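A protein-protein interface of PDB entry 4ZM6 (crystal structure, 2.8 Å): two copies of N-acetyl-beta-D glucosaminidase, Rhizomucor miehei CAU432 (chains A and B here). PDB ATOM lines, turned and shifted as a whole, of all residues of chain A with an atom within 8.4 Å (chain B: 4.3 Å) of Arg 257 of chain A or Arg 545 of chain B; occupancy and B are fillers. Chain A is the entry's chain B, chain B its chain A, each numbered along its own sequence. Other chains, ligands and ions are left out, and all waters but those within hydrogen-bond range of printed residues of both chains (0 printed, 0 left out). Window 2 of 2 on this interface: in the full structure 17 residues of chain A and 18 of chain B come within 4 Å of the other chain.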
ATOM      1  N   LYS A 214      21.666  33.980 -20.267  1.00  0.00           N
ATOM      2  CA  LYS A 214      22.972  34.342 -20.812  1.00  0.00           C
ATOM      3  C   LYS A 214      23.649  35.417 -19.956  1.00  0.00           C
ATOM      4  O   LYS A 214      24.821  35.280 -19.598  1.00  0.00           O
ATOM      5  CB  LYS A 214      22.847  34.833 -22.253  1.00  0.00           C
ATOM      6  CG  LYS A 214      24.189  35.021 -22.947  1.00  0.00           C
ATOM      7  CD  LYS A 214      24.098  36.049 -24.061  1.00  0.00           C
ATOM      8  CE  LYS A 214      25.423  36.196 -24.793  1.00  0.00           C
ATOM      9  NZ  LYS A 214      25.232  36.753 -26.158  1.00  0.00           N
ATOM     10  N   GLU A 218      27.206  34.755 -17.934  1.00  0.00           N
ATOM     11  CA  GLU A 218      28.401  35.536 -18.267  1.00  0.00           C
ATOM     12  C   GLU A 218      28.836  36.518 -17.173  1.00  0.00           C
ATOM     13  O   GLU A 218      29.850  37.195 -17.328  1.00  0.00           O
ATOM     14  CB  GLU A 218      28.167  36.310 -19.564  1.00  0.00           C
ATOM     15  CG  GLU A 218      27.989  35.420 -20.780  1.00  0.00           C
ATOM     16  CD  GLU A 218      27.677  36.203 -22.036  1.00  0.00           C
ATOM     17  OE1 GLU A 218      27.915  35.655 -23.132  1.00  0.00           O
ATOM     18  OE2 GLU A 218      27.197  37.357 -21.929  1.00  0.00           O
ATOM     19  N   PRO A 248      18.696  15.723 -24.544  1.00  0.00           N
ATOM     20  CA  PRO A 248      20.096  16.169 -24.626  1.00  0.00           C
ATOM     21  C   PRO A 248      20.305  17.383 -25.539  1.00  0.00           C
ATOM     22  O   PRO A 248      21.323  18.067 -25.433  1.00  0.00           O
ATOM     23  CB  PRO A 248      20.821  14.941 -25.186  1.00  0.00           C
ATOM     24  CG  PRO A 248      19.783  14.229 -25.973  1.00  0.00           C
ATOM     25  CD  PRO A 248      18.496  14.431 -25.224  1.00  0.00           C
ATOM     26  N   GLU A 249      19.341  17.641 -26.418  1.00  0.00           N
ATOM     27  CA  GLU A 249      19.379  18.794 -27.311  1.00  0.00           C
ATOM     28  C   GLU A 249      19.241  20.121 -26.545  1.00  0.00           C
ATOM     29  O   GLU A 249      19.648  21.172 -27.036  1.00  0.00           O
ATOM     30  CB  GLU A 249      18.277  18.678 -28.373  1.00  0.00           C
ATOM     31  CG  GLU A 249      18.416  17.476 -29.310  1.00  0.00           C
ATOM     32  CD  GLU A 249      17.701  16.213 -28.833  1.00  0.00           C
ATOM     33  OE1 GLU A 249      17.678  15.219 -29.594  1.00  0.00           O
ATOM     34  OE2 GLU A 249      17.166  16.198 -27.704  1.00  0.00           O
ATOM     35  N   ILE A 250      18.657  20.062 -25.350  1.00  0.00           N
ATOM     36  CA  ILE A 250      18.514  21.227 -24.478  1.00  0.00           C
ATOM     37  C   ILE A 250      19.606  21.278 -23.414  1.00  0.00           C
ATOM     38  O   ILE A 250      20.209  22.326 -23.182  1.00  0.00           O
ATOM     39  CB  ILE A 250      17.155  21.200 -23.753  1.00  0.00           C
ATOM     40  CG1 ILE A 250      16.001  21.331 -24.761  1.00  0.00           C
ATOM     41  CG2 ILE A 250      17.083  22.286 -22.684  1.00  0.00           C
ATOM     42  CD1 ILE A 250      15.890  22.681 -25.441  1.00  0.00           C
ATOM     43  N   VAL A 251      19.845  20.152 -22.756  1.00  0.00           N
ATOM     44  CA  VAL A 251      20.754  20.111 -21.619  1.00  0.00           C
ATOM     45  C   VAL A 251      22.216  20.184 -22.059  1.00  0.00           C
ATOM     46  O   VAL A 251      22.901  21.153 -21.753  1.00  0.00           O
ATOM     47  CB  VAL A 251      20.494  18.865 -20.755  1.00  0.00           C
ATOM     48  CG1 VAL A 251      21.525  18.749 -19.636  1.00  0.00           C
ATOM     49  CG2 VAL A 251      19.081  18.924 -20.186  1.00  0.00           C
ATOM     50  N   ARG A 252      22.697  19.174 -22.777  1.00  0.00           N
ATOM     51  CA  ARG A 252      24.102  19.157 -23.181  1.00  0.00           C
ATOM     52  C   ARG A 252      24.386  20.098 -24.356  1.00  0.00           C
ATOM     53  O   ARG A 252      25.279  20.945 -24.279  1.00  0.00           O
ATOM     54  CB  ARG A 252      24.558  17.739 -23.518  1.00  0.00           C
ATOM     55  CG  ARG A 252      26.042  17.645 -23.846  1.00  0.00           C
ATOM     56  CD  ARG A 252      26.596  16.245 -23.640  1.00  0.00           C
ATOM     57  NE  ARG A 252      25.601  15.225 -23.976  1.00  0.00           N
ATOM     58  CZ  ARG A 252      25.078  14.342 -23.126  1.00  0.00           C
ATOM     59  NH1 ARG A 252      25.459  14.292 -21.849  1.00  0.00           N
ATOM     60  NH2 ARG A 252      24.168  13.480 -23.569  1.00  0.00           N
ATOM     61  N   ASP A 253      23.619  19.951 -25.433  1.00  0.00           N
ATOM     62  CA  ASP A 253      23.858  20.714 -26.661  1.00  0.00           C
ATOM     63  C   ASP A 253      23.749  22.222 -26.469  1.00  0.00           C
ATOM     64  O   ASP A 253      24.528  22.977 -27.047  1.00  0.00           O
ATOM     65  CB  ASP A 253      22.890  20.280 -27.766  1.00  0.00           C
ATOM     66  CG  ASP A 253      23.185  18.888 -28.293  1.00  0.00           C
ATOM     67  OD1 ASP A 253      24.125  18.233 -27.787  1.00  0.00           O
ATOM     68  OD2 ASP A 253      22.468  18.450 -29.219  1.00  0.00           O
ATOM     69  N   LEU A 254      22.786  22.658 -25.664  1.00  0.00           N
ATOM     70  CA  LEU A 254      22.510  24.083 -25.519  1.00  0.00           C
ATOM     71  C   LEU A 254      23.218  24.681 -24.312  1.00  0.00           C
ATOM     72  O   LEU A 254      23.934  25.673 -24.443  1.00  0.00           O
ATOM     73  CB  LEU A 254      21.003  24.323 -25.411  1.00  0.00           C
ATOM     74  CG  LEU A 254      20.505  25.685 -25.884  1.00  0.00           C
ATOM     75  CD1 LEU A 254      20.624  25.790 -27.395  1.00  0.00           C
ATOM     76  CD2 LEU A 254      19.065  25.913 -25.448  1.00  0.00           C
ATOM     77  N   LEU A 255      23.021  24.078 -23.144  1.00  0.00           N
ATOM     78  CA  LEU A 255      23.565  24.625 -21.903  1.00  0.00           C
ATOM     79  C   LEU A 255      25.049  24.325 -21.745  1.00  0.00           C
ATOM     80  O   LEU A 255      25.829  25.212 -21.404  1.00  0.00           O
ATOM     81  CB  LEU A 255      22.795  24.089 -20.693  1.00  0.00           C
ATOM     82  CG  LEU A 255      22.924  24.845 -19.370  1.00  0.00           C
ATOM     83  CD1 LEU A 255      22.676  26.337 -19.537  1.00  0.00           C
ATOM     84  CD2 LEU A 255      21.959  24.262 -18.349  1.00  0.00           C
ATOM     85  N   ARG A 256      25.443  23.080 -21.994  1.00  0.00           N
ATOM     86  CA  ARG A 256      26.827  22.667 -21.755  1.00  0.00           C
ATOM     87  C   ARG A 256      27.761  23.041 -22.904  1.00  0.00           C
ATOM     88  O   ARG A 256      28.844  23.564 -22.668  1.00  0.00           O
ATOM     89  CB  ARG A 256      26.907  21.161 -21.462  1.00  0.00           C
ATOM     90  CG  ARG A 256      28.195  20.720 -20.777  1.00  0.00           C
ATOM     91  CD  ARG A 256      28.306  21.251 -19.351  1.00  0.00           C
ATOM     92  NE  ARG A 256      27.571  20.439 -18.379  1.00  0.00           N
ATOM     93  CZ  ARG A 256      27.350  20.784 -17.110  1.00  0.00           C
ATOM     94  NH1 ARG A 256      27.785  21.945 -16.625  1.00  0.00           N
ATOM     95  NH2 ARG A 256      26.674  19.963 -16.317  1.00  0.00           N
ATOM     96  N   ARG A 257      27.342  22.776 -24.140  1.00  0.00           N
ATOM     97  CA  ARG A 257      28.191  23.031 -25.308  1.00  0.00           C
ATOM     98  C   ARG A 257      28.117  24.488 -25.768  1.00  0.00           C
ATOM     99  O   ARG A 257      29.126  25.195 -25.756  1.00  0.00           O
ATOM    100  CB  ARG A 257      27.847  22.073 -26.460  1.00  0.00           C
ATOM    101  CG  ARG A 257      28.547  22.400 -27.778  1.00  0.00           C
ATOM    102  CD  ARG A 257      28.833  21.176 -28.649  1.00  0.00           C
ATOM    103  NE  ARG A 257      27.804  20.137 -28.538  1.00  0.00           N
ATOM    104  CZ  ARG A 257      28.017  18.870 -28.177  1.00  0.00           C
ATOM    105  NH1 ARG A 257      29.240  18.422 -27.895  1.00  0.00           N
ATOM    106  NH2 ARG A 257      26.990  18.028 -28.106  1.00  0.00           N
ATOM    107  N   ARG A 258      26.926  24.929 -26.157  1.00  0.00           N
ATOM    108  CA  ARG A 258      26.746  26.252 -26.776  1.00  0.00           C
ATOM    109  C   ARG A 258      27.077  27.412 -25.835  1.00  0.00           C
ATOM    110  O   ARG A 258      27.779  28.343 -26.228  1.00  0.00           O
ATOM    111  CB  ARG A 258      25.333  26.374 -27.382  1.00  0.00           C
ATOM    112  CG  ARG A 258      24.538  27.633 -27.058  1.00  0.00           C
ATOM    113  CD  ARG A 258      24.865  28.823 -27.945  1.00  0.00           C
ATOM    114  NE  ARG A 258      23.829  29.853 -27.806  1.00  0.00           N
ATOM    115  CZ  ARG A 258      23.460  30.715 -28.755  1.00  0.00           C
ATOM    116  NH1 ARG A 258      24.033  30.711 -29.954  1.00  0.00           N
ATOM    117  NH2 ARG A 258      22.497  31.592 -28.509  1.00  0.00           N
ATOM    118  N   PHE A 259      26.577  27.354 -24.604  1.00  0.00           N
ATOM    119  CA  PHE A 259      26.870  28.384 -23.607  1.00  0.00           C
ATOM    120  C   PHE A 259      28.168  28.092 -22.851  1.00  0.00           C
ATOM    121  O   PHE A 259      28.756  28.993 -22.256  1.00  0.00           O
ATOM    122  CB  PHE A 259      25.720  28.527 -22.606  1.00  0.00           C
ATOM    123  CG  PHE A 259      24.541  29.298 -23.133  1.00  0.00           C
ATOM    124  CD1 PHE A 259      24.647  30.653 -23.408  1.00  0.00           C
ATOM    125  CD2 PHE A 259      23.318  28.676 -23.329  1.00  0.00           C
ATOM    126  CE1 PHE A 259      23.562  31.368 -23.888  1.00  0.00           C
ATOM    127  CE2 PHE A 259      22.232  29.386 -23.801  1.00  0.00           C
ATOM    128  CZ  PHE A 259      22.353  30.733 -24.084  1.00  0.00           C
ATOM    129  N   GLY A 260      28.607  26.838 -22.856  1.00  0.00           N
ATOM    130  CA  GLY A 260      29.852  26.471 -22.194  1.00  0.00           C
ATOM    131  C   GLY A 260      29.813  26.626 -20.683  1.00  0.00           C
ATOM    132  O   GLY A 260      30.821  26.977 -20.068  1.00  0.00           O
ATOM    133  N   TYR A 261      28.654  26.363 -20.086  1.00  0.00           N
ATOM    134  CA  TYR A 261      28.490  26.454 -18.636  1.00  0.00           C
ATOM    135  C   TYR A 261      29.266  25.348 -17.929  1.00  0.00           C
ATOM    136  O   TYR A 261      29.193  24.185 -18.323  1.00  0.00           O
ATOM    137  CB  TYR A 261      27.013  26.340 -18.277  1.00  0.00           C
ATOM    138  CG  TYR A 261      26.708  26.521 -16.813  1.00  0.00           C
ATOM    139  CD1 TYR A 261      27.020  27.707 -16.161  1.00  0.00           C
ATOM    140  CD2 TYR A 261      26.080  25.516 -16.085  1.00  0.00           C
ATOM    141  CE1 TYR A 261      26.725  27.888 -14.821  1.00  0.00           C
ATOM    142  CE2 TYR A 261      25.779  25.687 -14.743  1.00  0.00           C
ATOM    143  CZ  TYR A 261      26.103  26.874 -14.116  1.00  0.00           C
ATOM    144  OH  TYR A 261      25.809  27.042 -12.784  1.00  0.00           O
ATOM    145  N   LYS A 262      29.997  25.720 -16.879  1.00  0.00           N
ATOM    146  CA  LYS A 262      30.822  24.769 -16.127  1.00  0.00           C
ATOM    147  C   LYS A 262      30.237  24.387 -14.770  1.00  0.00           C
ATOM    148  O   LYS A 262      30.783  23.518 -14.093  1.00  0.00           O
ATOM    149  CB  LYS A 262      32.226  25.341 -15.918  1.00  0.00           C
ATOM    150  CG  LYS A 262      32.948  25.720 -17.201  1.00  0.00           C
ATOM    151  CD  LYS A 262      32.960  24.581 -18.213  1.00  0.00           C
ATOM    152  CE  LYS A 262      33.965  24.834 -19.329  1.00  0.00           C
ATOM    153  NZ  LYS A 262      33.807  26.182 -19.947  1.00  0.00           N
ATOM    154  N   ILE A 265      24.179  21.416 -13.336  1.00  0.00           N
ATOM    155  CA  ILE A 265      22.854  21.416 -13.949  1.00  0.00           C
ATOM    156  C   ILE A 265      21.963  20.427 -13.197  1.00  0.00           C
ATOM    157  O   ILE A 265      22.333  19.266 -12.997  1.00  0.00           O
ATOM    158  CB  ILE A 265      22.901  21.032 -15.441  1.00  0.00           C
ATOM    159  CG1 ILE A 265      23.928  21.892 -16.191  1.00  0.00           C
ATOM    160  CG2 ILE A 265      21.516  21.181 -16.072  1.00  0.00           C
ATOM    161  CD1 ILE A 265      24.153  21.466 -17.626  1.00  0.00           C
ATOM    162  N   ALA A 291      20.758  12.787 -20.481  1.00  0.00           N
ATOM    163  CA  ALA A 291      20.637  14.059 -21.205  1.00  0.00           C
ATOM    164  C   ALA A 291      21.799  15.021 -20.928  1.00  0.00           C
ATOM    165  O   ALA A 291      22.076  15.910 -21.738  1.00  0.00           O
ATOM    166  CB  ALA A 291      19.315  14.736 -20.870  1.00  0.00           C
ATOM    167  N   ASP B 543      30.148  34.793 -29.934  1.00  0.00           N
ATOM    168  CA  ASP B 543      31.518  35.207 -29.679  1.00  0.00           C
ATOM    169  C   ASP B 543      32.381  33.975 -29.475  1.00  0.00           C
ATOM    170  O   ASP B 543      31.967  33.010 -28.830  1.00  0.00           O
ATOM    171  CB  ASP B 543      31.594  36.114 -28.453  1.00  0.00           C
ATOM    172  CG  ASP B 543      30.996  37.484 -28.704  1.00  0.00           C
ATOM    173  OD1 ASP B 543      31.253  38.058 -29.780  1.00  0.00           O
ATOM    174  OD2 ASP B 543      30.269  37.995 -27.827  1.00  0.00           O
ATOM    175  N   TYR B 544      33.573  34.012 -30.051  1.00  0.00           N
ATOM    176  CA  TYR B 544      34.549  32.949 -29.882  1.00  0.00           C
ATOM    177  C   TYR B 544      35.037  32.937 -28.432  1.00  0.00           C
ATOM    178  O   TYR B 544      35.376  33.985 -27.876  1.00  0.00           O
ATOM    179  CB  TYR B 544      35.714  33.160 -30.862  1.00  0.00           C
ATOM    180  CG  TYR B 544      36.942  32.306 -30.614  1.00  0.00           C
ATOM    181  CD1 TYR B 544      36.933  30.942 -30.879  1.00  0.00           C
ATOM    182  CD2 TYR B 544      38.122  32.874 -30.140  1.00  0.00           C
ATOM    183  CE1 TYR B 544      38.060  30.166 -30.662  1.00  0.00           C
ATOM    184  CE2 TYR B 544      39.249  32.107 -29.927  1.00  0.00           C
ATOM    185  CZ  TYR B 544      39.214  30.758 -30.186  1.00  0.00           C
ATOM    186  OH  TYR B 544      40.341  30.002 -29.961  1.00  0.00           O
ATOM    187  N   ARG B 545      35.031  31.753 -27.822  1.00  0.00           N
ATOM    188  CA  ARG B 545      35.560  31.554 -26.476  1.00  0.00           C
ATOM    189  C   ARG B 545      36.723  30.582 -26.584  1.00  0.00           C
ATOM    190  O   ARG B 545      36.524  29.390 -26.830  1.00  0.00           O
ATOM    191  CB  ARG B 545      34.489  30.990 -25.536  1.00  0.00           C
ATOM    192  CG  ARG B 545      33.256  31.870 -25.379  1.00  0.00           C
ATOM    193  CD  ARG B 545      32.329  31.365 -24.277  1.00  0.00           C
ATOM    194  NE  ARG B 545      31.917  29.967 -24.462  1.00  0.00           N
ATOM    195  CZ  ARG B 545      30.899  29.552 -25.220  1.00  0.00           C
ATOM    196  NH1 ARG B 545      30.154  30.415 -25.908  1.00  0.00           N
ATOM    197  NH2 ARG B 545      30.624  28.255 -25.296  1.00  0.00           N
ATOM    198  N   ASN B 546      37.938  31.095 -26.413  1.00  0.00           N
ATOM    199  CA  ASN B 546      39.139  30.289 -26.623  1.00  0.00           C
ATOM    200  C   ASN B 546      39.241  29.058 -25.709  1.00  0.00           C
ATOM    201  O   ASN B 546      39.761  28.022 -26.126  1.00  0.00           O
ATOM    202  CB  ASN B 546      40.407  31.158 -26.549  1.00  0.00           C
ATOM    203  CG  ASN B 546      40.656  31.735 -25.165  1.00  0.00           C
ATOM    204  OD1 ASN B 546      39.778  32.358 -24.569  1.00  0.00           O
ATOM    205  ND2 ASN B 546      41.867  31.543 -24.658  1.00  0.00           N
ATOM    206  N   ASP B 547      38.722  29.151 -24.488  1.00  0.00           N
ATOM    207  CA  ASP B 547      38.739  28.005 -23.575  1.00  0.00           C
ATOM    208  C   ASP B 547      37.924  26.823 -24.102  1.00  0.00           C
ATOM    209  O   ASP B 547      38.330  25.673 -23.949  1.00  0.00           O
ATOM    210  CB  ASP B 547      38.240  28.403 -22.183  1.00  0.00           C
ATOM    211  CG  ASP B 547      39.208  29.342 -21.452  1.00  0.00           C
ATOM    212  OD1 ASP B 547      40.425  29.335 -21.762  1.00  0.00           O
ATOM    213  OD2 ASP B 547      38.748  30.086 -20.557  1.00  0.00           O
ATOM    214  N   ASP B 548      36.790  27.107 -24.739  1.00  0.00           N
ATOM    215  CA  ASP B 548      35.874  26.066 -25.213  1.00  0.00           C
ATOM    216  C   ASP B 548      36.026  25.708 -26.694  1.00  0.00           C
ATOM    217  O   ASP B 548      35.805  24.561 -27.075  1.00  0.00           O
ATOM    218  CB  ASP B 548      34.429  26.504 -24.960  1.00  0.00           C
ATOM    219  CG  ASP B 548      34.147  26.774 -23.496  1.00  0.00           C
ATOM    220  OD1 ASP B 548      34.625  25.985 -22.650  1.00  0.00           O
ATOM    221  OD2 ASP B 548      33.448  27.769 -23.190  1.00  0.00           O
ATOM    222  N   ASP B 549      36.395  26.684 -27.523  1.00  0.00           N
ATOM    223  CA  ASP B 549      36.303  26.546 -28.983  1.00  0.00           C
ATOM    224  C   ASP B 549      37.626  26.284 -29.714  1.00  0.00           C
ATOM    225  O   ASP B 549      37.622  25.985 -30.912  1.00  0.00           O
ATOM    226  CB  ASP B 549      35.664  27.807 -29.567  1.00  0.00           C
ATOM    227  CG  ASP B 549      34.308  28.119 -28.954  1.00  0.00           C
ATOM    228  OD1 ASP B 549      33.631  27.182 -28.465  1.00  0.00           O
ATOM    229  OD2 ASP B 549      33.918  29.310 -28.968  1.00  0.00           O
ATOM    230  N   ARG B 588      27.441  28.242 -35.161  1.00  0.00           N
ATOM    231  CA  ARG B 588      26.969  26.967 -34.622  1.00  0.00           C
ATOM    232  C   ARG B 588      25.626  26.579 -35.231  1.00  0.00           C
ATOM    233  O   ARG B 588      24.785  27.442 -35.479  1.00  0.00           O
ATOM    234  CB  ARG B 588      26.788  27.058 -33.106  1.00  0.00           C
ATOM    235  CG  ARG B 588      28.039  27.359 -32.301  1.00  0.00           C
ATOM    236  CD  ARG B 588      27.710  27.389 -30.815  1.00  0.00           C
ATOM    237  NE  ARG B 588      28.713  28.106 -30.024  1.00  0.00           N
ATOM    238  CZ  ARG B 588      29.789  27.561 -29.448  1.00  0.00           C
ATOM    239  NH1 ARG B 588      30.045  26.264 -29.560  1.00  0.00           N
ATOM    240  NH2 ARG B 588      30.622  28.330 -28.752  1.00  0.00           N
ATOM    241  N   GLN B 591      22.314  22.387 -32.750  1.00  0.00           N
ATOM    242  CA  GLN B 591      22.900  21.524 -31.714  1.00  0.00           C
ATOM    243  C   GLN B 591      24.234  22.033 -31.133  1.00  0.00           C
ATOM    244  O   GLN B 591      24.930  21.291 -30.433  1.00  0.00           O
ATOM    245  CB  GLN B 591      23.092  20.112 -32.275  1.00  0.00           C
ATOM    246  CG  GLN B 591      21.788  19.431 -32.653  1.00  0.00           C
ATOM    247  CD  GLN B 591      22.004  18.057 -33.260  1.00  0.00           C
ATOM    248  OE1 GLN B 591      22.832  17.888 -34.154  1.00  0.00           O
ATOM    249  NE2 GLN B 591      21.253  17.068 -32.782  1.00  0.00           N
ATOM    250  N   GLY B 592      24.588  23.287 -31.420  1.00  0.00           N
ATOM    251  CA  GLY B 592      25.766  23.925 -30.822  1.00  0.00           C
ATOM    252  C   GLY B 592      27.105  23.492 -31.392  1.00  0.00           C
ATOM    253  O   GLY B 592      28.159  23.843 -30.851  1.00  0.00           O
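The guanidinium group of Arg 545 of chain B lies within hydrogen-bond range of the backbone carbonyl oxygen of Arg 257 of chain A (3.4 Å).
The guanidinium group (NH2) of Arg 545 of chain B sits at hydrogen-bond distance from the backbone carbonyl oxygen (O) of Arg 258 of chain A, 3.0 Å away.
The side-chain carboxylate (OD1) of Asp 548 of chain B is in salt-bridge range of the side-chain amino group (NZ) of Lys 262 of chain A (2.8 Å).
The backbone NH (N) of Gly 260 of chain A sits close to the guanidinium group (NH2) of Arg 545 of chain B (3.5 Å).
Among the printed residues, pairs that only touch across the chains: Arg 257 of chain A with Gly 592 of chain B (3.4 Å), Phe 259 of chain A with Arg 545 of chain B (3.5 Å), Asp 253 of chain A with Gln 591 of chain B (3.5 Å), Arg 257 of chain A with Gln 591 of chain B (3.6 Å), Arg 258 of chain A with Arg 588 of chain B (3.8 Å) and Gly 260 of chain A with Asp 548 of chain B (3.95 Å).
No position is printed for both chains.
Glu 218 of chain A touches none of the printed residues of chain B.
Val 251 of chain A touches none of the printed residues of chain B.
Of the printed residues of chain B, Arg 258 of chain A touches Arg 545 and Arg 588.
Printed residues of chain B within 4 Å of Gly 260 of chain A: Arg 545 (3.5 Å) and Asp 548 (3.95 Å).
Printed residues of chain B within 4 Å of Lys 262 of chain A: Asp 548.
The nearest residue of chain B that does not touch Arg 257 of chain A is Arg 588 of chain B (4.1 Å).
The guanidinium group (NE) of Arg 545 of chain B lies within salt-bridge range of the side-chain carboxylate (OD2) of Asp 548 of chain B (3.0 Å).
The guanidinium group (NH1) of Arg 588 of chain B sits at hydrogen-bond distance from the backbone carbonyl oxygen (O) of Gly 592 of chain B, at 3.3 Å.
The backbone carbonyl oxygen (O) of Pro 248 of chain A is in hydrogen-bond range of the backbone NH (N) of Asp 253 of chain A (3.0 Å).
O of Arg 252 of chain A lies within hydrogen-bond range of N of Arg 257 of chain A.
NH2 of Arg 257 of chain A is in salt-bridge range of OD1 of Asp 253 of chain A.
The backbone carbonyl oxygen of Asp 253 of chain A lies within hydrogen-bond range of the backbone NH of Arg 258 of chain A (3.2 Å).
Printed residues of chain A that touch a printed residue of chain B: Asp 253, Arg 257, Arg 258, Phe 259, Gly 260 and Lys 262.
Of the 10 printed residues of chain B, 5 touch a printed residue of chain A.
Among the printed residues, 10 pairs touch across the chains.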
